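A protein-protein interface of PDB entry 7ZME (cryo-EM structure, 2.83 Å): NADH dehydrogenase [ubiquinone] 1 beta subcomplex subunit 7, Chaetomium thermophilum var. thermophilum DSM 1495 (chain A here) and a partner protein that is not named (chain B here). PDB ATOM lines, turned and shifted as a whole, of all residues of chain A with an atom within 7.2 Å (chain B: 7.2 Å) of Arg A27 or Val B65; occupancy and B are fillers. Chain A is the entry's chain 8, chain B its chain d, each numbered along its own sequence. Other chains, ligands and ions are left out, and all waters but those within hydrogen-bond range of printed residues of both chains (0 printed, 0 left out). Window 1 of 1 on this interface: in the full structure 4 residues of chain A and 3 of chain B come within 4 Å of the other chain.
Of the printed residues of chain B, Arg A18 touches Asn B66 (3.3 Å) and Glu B69 (3.2 Å).
Of the printed residues of chain B, Val A22 touches Val B65.
Of the printed residues of chain B, Leu A24 touches Val B65.
Printed residues of chain B within 4 Å of Arg A27: Val B65.
Asp A28 touches none of the printed residues of chain B.
Of the printed residues of chain A, Asn B66 touches Arg A18 (3.3 Å).
Leu B68 touches none of the printed residues of chain A.
Printed residues of chain A within 4 Å of Glu B69: Arg A18.
The nearest printed residue of chain B that does not touch Leu A24 is Asn B66 (5.5 Å).
The side-chain carboxylate (OE2) of Glu B69 is in salt-bridge range of the guanidinium group (NH2) of Arg A18, 3.5 Å away.
The side-chain carboxylate (OE1) of Glu B63 sits close to the side-chain amide oxygen (OD1) of Asn B66 (2.7 Å).
The side-chain carboxylate (OD1) of Asp A19 is in salt-bridge range of the guanidinium group (NE) of Arg A18 (3.2 Å).
The backbone carbonyl oxygen (O) of Val A22 is in hydrogen-bond range of the guanidinium group (NH2) of Arg A27, at 2.6 Å.
CG of Arg A18 touches ND2 of Asn B66, 3.3 Å away.
O of Val A22 touches CG1 of Val B65, at 3.4 Å.
CG1 of Val B65 touches CD2 of Leu A24 (3.4 Å).
Val B65 touches Arg A27.
Printed residues of chain B that touch a printed residue of chain A: Val B65, Asn B66 and Glu B69.
Hydrophobic or aromatic side chains of chain B that line the printed part of chain A: Val B65.
Hydrophobic or aromatic side chains of chain A that line the printed part of chain B: Leu A24.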
ATOM      1  N   ARG A  14     -15.745 -14.344 -25.579  1.00  0.00           N
ATOM      2  CA  ARG A  14     -14.754 -13.518 -26.264  1.00  0.00           C
ATOM      3  C   ARG A  14     -15.311 -12.159 -26.662  1.00  0.00           C
ATOM      4  O   ARG A  14     -14.561 -11.178 -26.723  1.00  0.00           O
ATOM      5  CB  ARG A  14     -14.239 -14.244 -27.505  1.00  0.00           C
ATOM      6  CG  ARG A  14     -13.455 -15.512 -27.223  1.00  0.00           C
ATOM      7  CD  ARG A  14     -13.017 -16.156 -28.526  1.00  0.00           C
ATOM      8  NE  ARG A  14     -12.259 -17.386 -28.315  1.00  0.00           N
ATOM      9  CZ  ARG A  14     -11.815 -18.162 -29.297  1.00  0.00           C
ATOM     10  NH1 ARG A  14     -11.134 -19.263 -29.016  1.00  0.00           N
ATOM     11  NH2 ARG A  14     -12.052 -17.838 -30.560  1.00  0.00           N
ATOM     12  N   MET A  17     -14.853  -9.950 -24.159  1.00  0.00           N
ATOM     13  CA  MET A  17     -13.501 -10.180 -23.676  1.00  0.00           C
ATOM     14  C   MET A  17     -12.442  -9.699 -24.659  1.00  0.00           C
ATOM     15  O   MET A  17     -11.312  -9.418 -24.244  1.00  0.00           O
ATOM     16  CB  MET A  17     -13.330 -11.671 -23.383  1.00  0.00           C
ATOM     17  CG  MET A  17     -12.029 -12.114 -22.795  1.00  0.00           C
ATOM     18  SD  MET A  17     -12.219 -13.877 -22.491  1.00  0.00           S
ATOM     19  CE  MET A  17     -10.604 -14.299 -21.902  1.00  0.00           C
ATOM     20  N   ARG A  18     -12.786  -9.598 -25.943  1.00  0.00           N
ATOM     21  CA  ARG A  18     -11.976  -8.811 -26.865  1.00  0.00           C
ATOM     22  C   ARG A  18     -12.180  -7.322 -26.620  1.00  0.00           C
ATOM     23  O   ARG A  18     -11.234  -6.534 -26.717  1.00  0.00           O
ATOM     24  CB  ARG A  18     -12.326  -9.176 -28.308  1.00  0.00           C
ATOM     25  CG  ARG A  18     -11.707  -8.266 -29.357  1.00  0.00           C
ATOM     26  CD  ARG A  18     -12.739  -7.322 -29.964  1.00  0.00           C
ATOM     27  NE  ARG A  18     -13.995  -7.997 -30.275  1.00  0.00           N
ATOM     28  CZ  ARG A  18     -14.218  -8.682 -31.391  1.00  0.00           C
ATOM     29  NH1 ARG A  18     -15.393  -9.263 -31.592  1.00  0.00           N
ATOM     30  NH2 ARG A  18     -13.268  -8.784 -32.310  1.00  0.00           N
ATOM     31  N   ASP A  19     -13.414  -6.925 -26.295  1.00  0.00           N
ATOM     32  CA  ASP A  19     -13.695  -5.525 -25.994  1.00  0.00           C
ATOM     33  C   ASP A  19     -13.010  -5.080 -24.709  1.00  0.00           C
ATOM     34  O   ASP A  19     -12.656  -3.904 -24.572  1.00  0.00           O
ATOM     35  CB  ASP A  19     -15.203  -5.306 -25.890  1.00  0.00           C
ATOM     36  CG  ASP A  19     -15.892  -5.355 -27.240  1.00  0.00           C
ATOM     37  OD1 ASP A  19     -15.298  -5.903 -28.194  1.00  0.00           O
ATOM     38  OD2 ASP A  19     -17.029  -4.850 -27.350  1.00  0.00           O
ATOM     39  N   ALA A  20     -12.817  -5.997 -23.758  1.00  0.00           N
ATOM     40  CA  ALA A  20     -12.143  -5.654 -22.513  1.00  0.00           C
ATOM     41  C   ALA A  20     -10.649  -5.438 -22.703  1.00  0.00           C
ATOM     42  O   ALA A  20     -10.002  -4.875 -21.814  1.00  0.00           O
ATOM     43  CB  ALA A  20     -12.381  -6.744 -21.468  1.00  0.00           C
ATOM     44  N   LYS A  21     -10.093  -5.876 -23.836  1.00  0.00           N
ATOM     45  CA  LYS A  21      -8.678  -5.687 -24.160  1.00  0.00           C
ATOM     46  C   LYS A  21      -7.769  -6.296 -23.095  1.00  0.00           C
ATOM     47  O   LYS A  21      -6.835  -5.659 -22.607  1.00  0.00           O
ATOM     48  CB  LYS A  21      -8.354  -4.205 -24.367  1.00  0.00           C
ATOM     49  CG  LYS A  21      -9.026  -3.576 -25.574  1.00  0.00           C
ATOM     50  CD  LYS A  21      -8.639  -2.112 -25.712  1.00  0.00           C
ATOM     51  CE  LYS A  21      -9.233  -1.496 -26.966  1.00  0.00           C
ATOM     52  NZ  LYS A  21     -10.718  -1.414 -26.896  1.00  0.00           N
ATOM     53  N   VAL A  22      -8.049  -7.542 -22.727  1.00  0.00           N
ATOM     54  CA  VAL A  22      -7.168  -8.260 -21.810  1.00  0.00           C
ATOM     55  C   VAL A  22      -6.035  -8.877 -22.626  1.00  0.00           C
ATOM     56  O   VAL A  22      -6.202  -9.115 -23.830  1.00  0.00           O
ATOM     57  CB  VAL A  22      -7.938  -9.309 -20.989  1.00  0.00           C
ATOM     58  CG1 VAL A  22      -9.171  -8.683 -20.356  1.00  0.00           C
ATOM     59  CG2 VAL A  22      -8.315 -10.501 -21.836  1.00  0.00           C
ATOM     60  N   PRO A  23      -4.870  -9.124 -22.031  1.00  0.00           N
ATOM     61  CA  PRO A  23      -3.745  -9.671 -22.801  1.00  0.00           C
ATOM     62  C   PRO A  23      -4.026 -11.075 -23.322  1.00  0.00           C
ATOM     63  O   PRO A  23      -4.847 -11.817 -22.781  1.00  0.00           O
ATOM     64  CB  PRO A  23      -2.595  -9.670 -21.789  1.00  0.00           C
ATOM     65  CG  PRO A  23      -2.968  -8.591 -20.815  1.00  0.00           C
ATOM     66  CD  PRO A  23      -4.455  -8.685 -20.689  1.00  0.00           C
ATOM     67  N   LEU A  24      -3.323 -11.431 -24.403  1.00  0.00           N
ATOM     68  CA  LEU A  24      -3.563 -12.710 -25.065  1.00  0.00           C
ATOM     69  C   LEU A  24      -3.260 -13.881 -24.141  1.00  0.00           C
ATOM     70  O   LEU A  24      -4.033 -14.842 -24.063  1.00  0.00           O
ATOM     71  CB  LEU A  24      -2.718 -12.838 -26.331  1.00  0.00           C
ATOM     72  CG  LEU A  24      -3.166 -12.221 -27.655  1.00  0.00           C
ATOM     73  CD1 LEU A  24      -4.463 -12.860 -28.143  1.00  0.00           C
ATOM     74  CD2 LEU A  24      -3.261 -10.726 -27.590  1.00  0.00           C
ATOM     75  N   ALA A  25      -2.131 -13.821 -23.436  1.00  0.00           N
ATOM     76  CA  ALA A  25      -1.705 -14.937 -22.605  1.00  0.00           C
ATOM     77  C   ALA A  25      -2.632 -15.169 -21.424  1.00  0.00           C
ATOM     78  O   ALA A  25      -2.510 -16.199 -20.752  1.00  0.00           O
ATOM     79  CB  ALA A  25      -0.280 -14.706 -22.109  1.00  0.00           C
ATOM     80  N   TYR A  26      -3.548 -14.241 -21.154  1.00  0.00           N
ATOM     81  CA  TYR A  26      -4.497 -14.360 -20.058  1.00  0.00           C
ATOM     82  C   TYR A  26      -5.924 -14.536 -20.564  1.00  0.00           C
ATOM     83  O   TYR A  26      -6.880 -14.339 -19.808  1.00  0.00           O
ATOM     84  CB  TYR A  26      -4.379 -13.138 -19.151  1.00  0.00           C
ATOM     85  CG  TYR A  26      -3.045 -13.081 -18.450  1.00  0.00           C
ATOM     86  CD1 TYR A  26      -2.319 -14.239 -18.209  1.00  0.00           C
ATOM     87  CD2 TYR A  26      -2.482 -11.868 -18.087  1.00  0.00           C
ATOM     88  CE1 TYR A  26      -1.091 -14.195 -17.590  1.00  0.00           C
ATOM     89  CE2 TYR A  26      -1.249 -11.814 -17.471  1.00  0.00           C
ATOM     90  CZ  TYR A  26      -0.560 -12.980 -17.222  1.00  0.00           C
ATOM     91  OH  TYR A  26       0.667 -12.930 -16.606  1.00  0.00           O
ATOM     92  N   ARG A  27      -6.081 -14.905 -21.834  1.00  0.00           N
ATOM     93  CA  ARG A  27      -7.390 -15.188 -22.418  1.00  0.00           C
ATOM     94  C   ARG A  27      -7.790 -16.615 -22.054  1.00  0.00           C
ATOM     95  O   ARG A  27      -7.678 -17.554 -22.847  1.00  0.00           O
ATOM     96  CB  ARG A  27      -7.370 -14.992 -23.927  1.00  0.00           C
ATOM     97  CG  ARG A  27      -7.033 -13.593 -24.402  1.00  0.00           C
ATOM     98  CD  ARG A  27      -8.280 -12.817 -24.755  1.00  0.00           C
ATOM     99  NE  ARG A  27      -8.018 -11.386 -24.833  1.00  0.00           N
ATOM    100  CZ  ARG A  27      -7.904 -10.707 -25.967  1.00  0.00           C
ATOM    101  NH1 ARG A  27      -8.035 -11.327 -27.131  1.00  0.00           N
ATOM    102  NH2 ARG A  27      -7.663  -9.405 -25.935  1.00  0.00           N
ATOM    103  N   ASP A  28      -8.271 -16.779 -20.825  1.00  0.00           N
ATOM    104  CA  ASP A  28      -8.689 -18.100 -20.373  1.00  0.00           C
ATOM    105  C   ASP A  28      -9.932 -18.024 -19.494  1.00  0.00           C
ATOM    106  O   ASP A  28     -10.588 -16.980 -19.424  1.00  0.00           O
ATOM    107  CB  ASP A  28      -7.541 -18.795 -19.640  1.00  0.00           C
ATOM    108  CG  ASP A  28      -7.265 -18.195 -18.284  1.00  0.00           C
ATOM    109  OD1 ASP A  28      -7.306 -16.952 -18.159  1.00  0.00           O
ATOM    110  OD2 ASP A  28      -6.992 -18.970 -17.344  1.00  0.00           O
ATOM    111  N   SER A  29     -10.263 -19.134 -18.827  1.00  0.00           N
ATOM    112  CA  SER A  29     -11.534 -19.237 -18.116  1.00  0.00           C
ATOM    113  C   SER A  29     -11.637 -18.216 -16.988  1.00  0.00           C
ATOM    114  O   SER A  29     -12.669 -17.553 -16.830  1.00  0.00           O
ATOM    115  CB  SER A  29     -11.707 -20.654 -17.569  1.00  0.00           C
ATOM    116  OG  SER A  29     -10.744 -20.934 -16.568  1.00  0.00           O
ATOM    117  N   CYS A  30     -10.578 -18.074 -16.195  1.00  0.00           N
ATOM    118  CA  CYS A  30     -10.605 -17.207 -15.024  1.00  0.00           C
ATOM    119  C   CYS A  30     -10.642 -15.725 -15.368  1.00  0.00           C
ATOM    120  O   CYS A  30     -10.876 -14.912 -14.468  1.00  0.00           O
ATOM    121  CB  CYS A  30      -9.393 -17.494 -14.142  1.00  0.00           C
ATOM    122  SG  CYS A  30      -7.829 -17.261 -14.992  1.00  0.00           S
ATOM    123  N   ALA A  31     -10.419 -15.350 -16.628  1.00  0.00           N
ATOM    124  CA  ALA A  31     -10.314 -13.941 -16.990  1.00  0.00           C
ATOM    125  C   ALA A  31     -11.596 -13.161 -16.744  1.00  0.00           C
ATOM    126  O   ALA A  31     -11.587 -11.935 -16.890  1.00  0.00           O
ATOM    127  CB  ALA A  31      -9.904 -13.808 -18.456  1.00  0.00           C
ATOM    128  N   LEU A  34     -10.545 -11.181 -14.266  1.00  0.00           N
ATOM    129  CA  LEU A  34      -9.455 -10.304 -14.677  1.00  0.00           C
ATOM    130  C   LEU A  34      -9.976  -8.944 -15.119  1.00  0.00           C
ATOM    131  O   LEU A  34      -9.325  -7.919 -14.885  1.00  0.00           O
ATOM    132  CB  LEU A  34      -8.645 -10.957 -15.795  1.00  0.00           C
ATOM    133  CG  LEU A  34      -7.425 -10.180 -16.290  1.00  0.00           C
ATOM    134  CD1 LEU A  34      -6.411 -10.009 -15.181  1.00  0.00           C
ATOM    135  CD2 LEU A  34      -6.803 -10.882 -17.480  1.00  0.00           C
ATOM    136  N   TYR B  60      -3.291  -0.581 -36.446  1.00  0.00           N
ATOM    137  CA  TYR B  60      -2.434  -1.227 -35.458  1.00  0.00           C
ATOM    138  C   TYR B  60      -2.437  -0.473 -34.133  1.00  0.00           C
ATOM    139  O   TYR B  60      -2.595  -1.073 -33.065  1.00  0.00           O
ATOM    140  CB  TYR B  60      -1.015  -1.338 -36.011  1.00  0.00           C
ATOM    141  CG  TYR B  60      -0.042  -1.974 -35.059  1.00  0.00           C
ATOM    142  CD1 TYR B  60      -0.050  -3.340 -34.854  1.00  0.00           C
ATOM    143  CD2 TYR B  60       0.876  -1.207 -34.359  1.00  0.00           C
ATOM    144  CE1 TYR B  60       0.828  -3.927 -33.985  1.00  0.00           C
ATOM    145  CE2 TYR B  60       1.762  -1.788 -33.485  1.00  0.00           C
ATOM    146  CZ  TYR B  60       1.732  -3.151 -33.302  1.00  0.00           C
ATOM    147  OH  TYR B  60       2.612  -3.753 -32.436  1.00  0.00           O
ATOM    148  N   ARG B  62      -4.681   1.704 -33.251  1.00  0.00           N
ATOM    149  CA  ARG B  62      -6.054   1.807 -32.777  1.00  0.00           C
ATOM    150  C   ARG B  62      -6.466   0.568 -31.993  1.00  0.00           C
ATOM    151  O   ARG B  62      -7.146   0.673 -30.967  1.00  0.00           O
ATOM    152  CB  ARG B  62      -6.993   2.027 -33.960  1.00  0.00           C
ATOM    153  CG  ARG B  62      -8.438   2.273 -33.582  1.00  0.00           C
ATOM    154  CD  ARG B  62      -9.271   2.545 -34.816  1.00  0.00           C
ATOM    155  NE  ARG B  62      -9.320   1.381 -35.694  1.00  0.00           N
ATOM    156  CZ  ARG B  62      -8.777   1.338 -36.905  1.00  0.00           C
ATOM    157  NH1 ARG B  62      -8.869   0.234 -37.636  1.00  0.00           N
ATOM    158  NH2 ARG B  62      -8.146   2.398 -37.390  1.00  0.00           N
ATOM    159  N   GLU B  63      -6.069  -0.614 -32.457  1.00  0.00           N
ATOM    160  CA  GLU B  63      -6.565  -1.850 -31.865  1.00  0.00           C
ATOM    161  C   GLU B  63      -5.696  -2.325 -30.704  1.00  0.00           C
ATOM    162  O   GLU B  63      -6.218  -2.678 -29.643  1.00  0.00           O
ATOM    163  CB  GLU B  63      -6.666  -2.939 -32.935  1.00  0.00           C
ATOM    164  CG  GLU B  63      -7.876  -2.797 -33.846  1.00  0.00           C
ATOM    165  CD  GLU B  63      -9.132  -2.358 -33.114  1.00  0.00           C
ATOM    166  OE1 GLU B  63      -9.512  -3.003 -32.116  1.00  0.00           O
ATOM    167  OE2 GLU B  63      -9.742  -1.354 -33.537  1.00  0.00           O
ATOM    168  N   GLY B  64      -4.381  -2.345 -30.885  1.00  0.00           N
ATOM    169  CA  GLY B  64      -3.485  -2.733 -29.814  1.00  0.00           C
ATOM    170  C   GLY B  64      -3.383  -4.230 -29.606  1.00  0.00           C
ATOM    171  O   GLY B  64      -2.759  -4.933 -30.403  1.00  0.00           O
ATOM    172  N   VAL B  65      -3.976  -4.719 -28.517  1.00  0.00           N
ATOM    173  CA  VAL B  65      -3.996  -6.155 -28.251  1.00  0.00           C
ATOM    174  C   VAL B  65      -4.672  -6.900 -29.389  1.00  0.00           C
ATOM    175  O   VAL B  65      -4.128  -7.866 -29.937  1.00  0.00           O
ATOM    176  CB  VAL B  65      -4.700  -6.433 -26.911  1.00  0.00           C
ATOM    177  CG1 VAL B  65      -4.832  -7.901 -26.684  1.00  0.00           C
ATOM    178  CG2 VAL B  65      -3.902  -5.863 -25.800  1.00  0.00           C
ATOM    179  N   ASN B  66      -5.865  -6.457 -29.765  1.00  0.00           N
ATOM    180  CA  ASN B  66      -6.653  -7.113 -30.803  1.00  0.00           C
ATOM    181  C   ASN B  66      -6.405  -6.524 -32.189  1.00  0.00           C
ATOM    182  O   ASN B  66      -7.331  -6.193 -32.921  1.00  0.00           O
ATOM    183  CB  ASN B  66      -8.128  -7.069 -30.417  1.00  0.00           C
ATOM    184  CG  ASN B  66      -8.674  -5.655 -30.326  1.00  0.00           C
ATOM    185  OD1 ASN B  66      -7.996  -4.687 -30.660  1.00  0.00           O
ATOM    186  ND2 ASN B  66      -9.913  -5.533 -29.866  1.00  0.00           N
ATOM    187  N   HIS B  67      -5.134  -6.414 -32.570  1.00  0.00           N
ATOM    188  CA  HIS B  67      -4.780  -6.074 -33.940  1.00  0.00           C
ATOM    189  C   HIS B  67      -4.609  -7.310 -34.801  1.00  0.00           C
ATOM    190  O   HIS B  67      -4.825  -7.250 -36.015  1.00  0.00           O
ATOM    191  CB  HIS B  67      -3.480  -5.265 -33.986  1.00  0.00           C
ATOM    192  CG  HIS B  67      -2.243  -6.090 -33.811  1.00  0.00           C
ATOM    193  ND1 HIS B  67      -1.548  -6.615 -34.878  1.00  0.00           N
ATOM    194  CD2 HIS B  67      -1.585  -6.496 -32.700  1.00  0.00           C
ATOM    195  CE1 HIS B  67      -0.510  -7.296 -34.435  1.00  0.00           C
ATOM    196  NE2 HIS B  67      -0.513  -7.245 -33.116  1.00  0.00           N
ATOM    197  N   LEU B  68      -4.231  -8.431 -34.184  1.00  0.00           N
ATOM    198  CA  LEU B  68      -4.033  -9.680 -34.898  1.00  0.00           C
ATOM    199  C   LEU B  68      -5.340 -10.298 -35.367  1.00  0.00           C
ATOM    200  O   LEU B  68      -5.307 -11.239 -36.165  1.00  0.00           O
ATOM    201  CB  LEU B  68      -3.272 -10.660 -34.009  1.00  0.00           C
ATOM    202  CG  LEU B  68      -1.752 -10.531 -34.073  1.00  0.00           C
ATOM    203  CD1 LEU B  68      -1.079 -11.598 -33.235  1.00  0.00           C
ATOM    204  CD2 LEU B  68      -1.285 -10.600 -35.517  1.00  0.00           C
ATOM    205  N   GLU B  69      -6.483  -9.792 -34.906  1.00  0.00           N
ATOM    206  CA  GLU B  69      -7.770 -10.286 -35.360  1.00  0.00           C
ATOM    207  C   GLU B  69      -8.688  -9.202 -35.895  1.00  0.00           C
ATOM    208  O   GLU B  69      -9.823  -9.511 -36.277  1.00  0.00           O
ATOM    209  CB  GLU B  69      -8.486 -11.038 -34.230  1.00  0.00           C
ATOM    210  CG  GLU B  69      -9.124 -10.154 -33.182  1.00  0.00           C
ATOM    211  CD  GLU B  69     -10.147 -10.900 -32.352  1.00  0.00           C
ATOM    212  OE1 GLU B  69     -10.682 -11.919 -32.840  1.00  0.00           O
ATOM    213  OE2 GLU B  69     -10.410 -10.477 -31.208  1.00  0.00           O
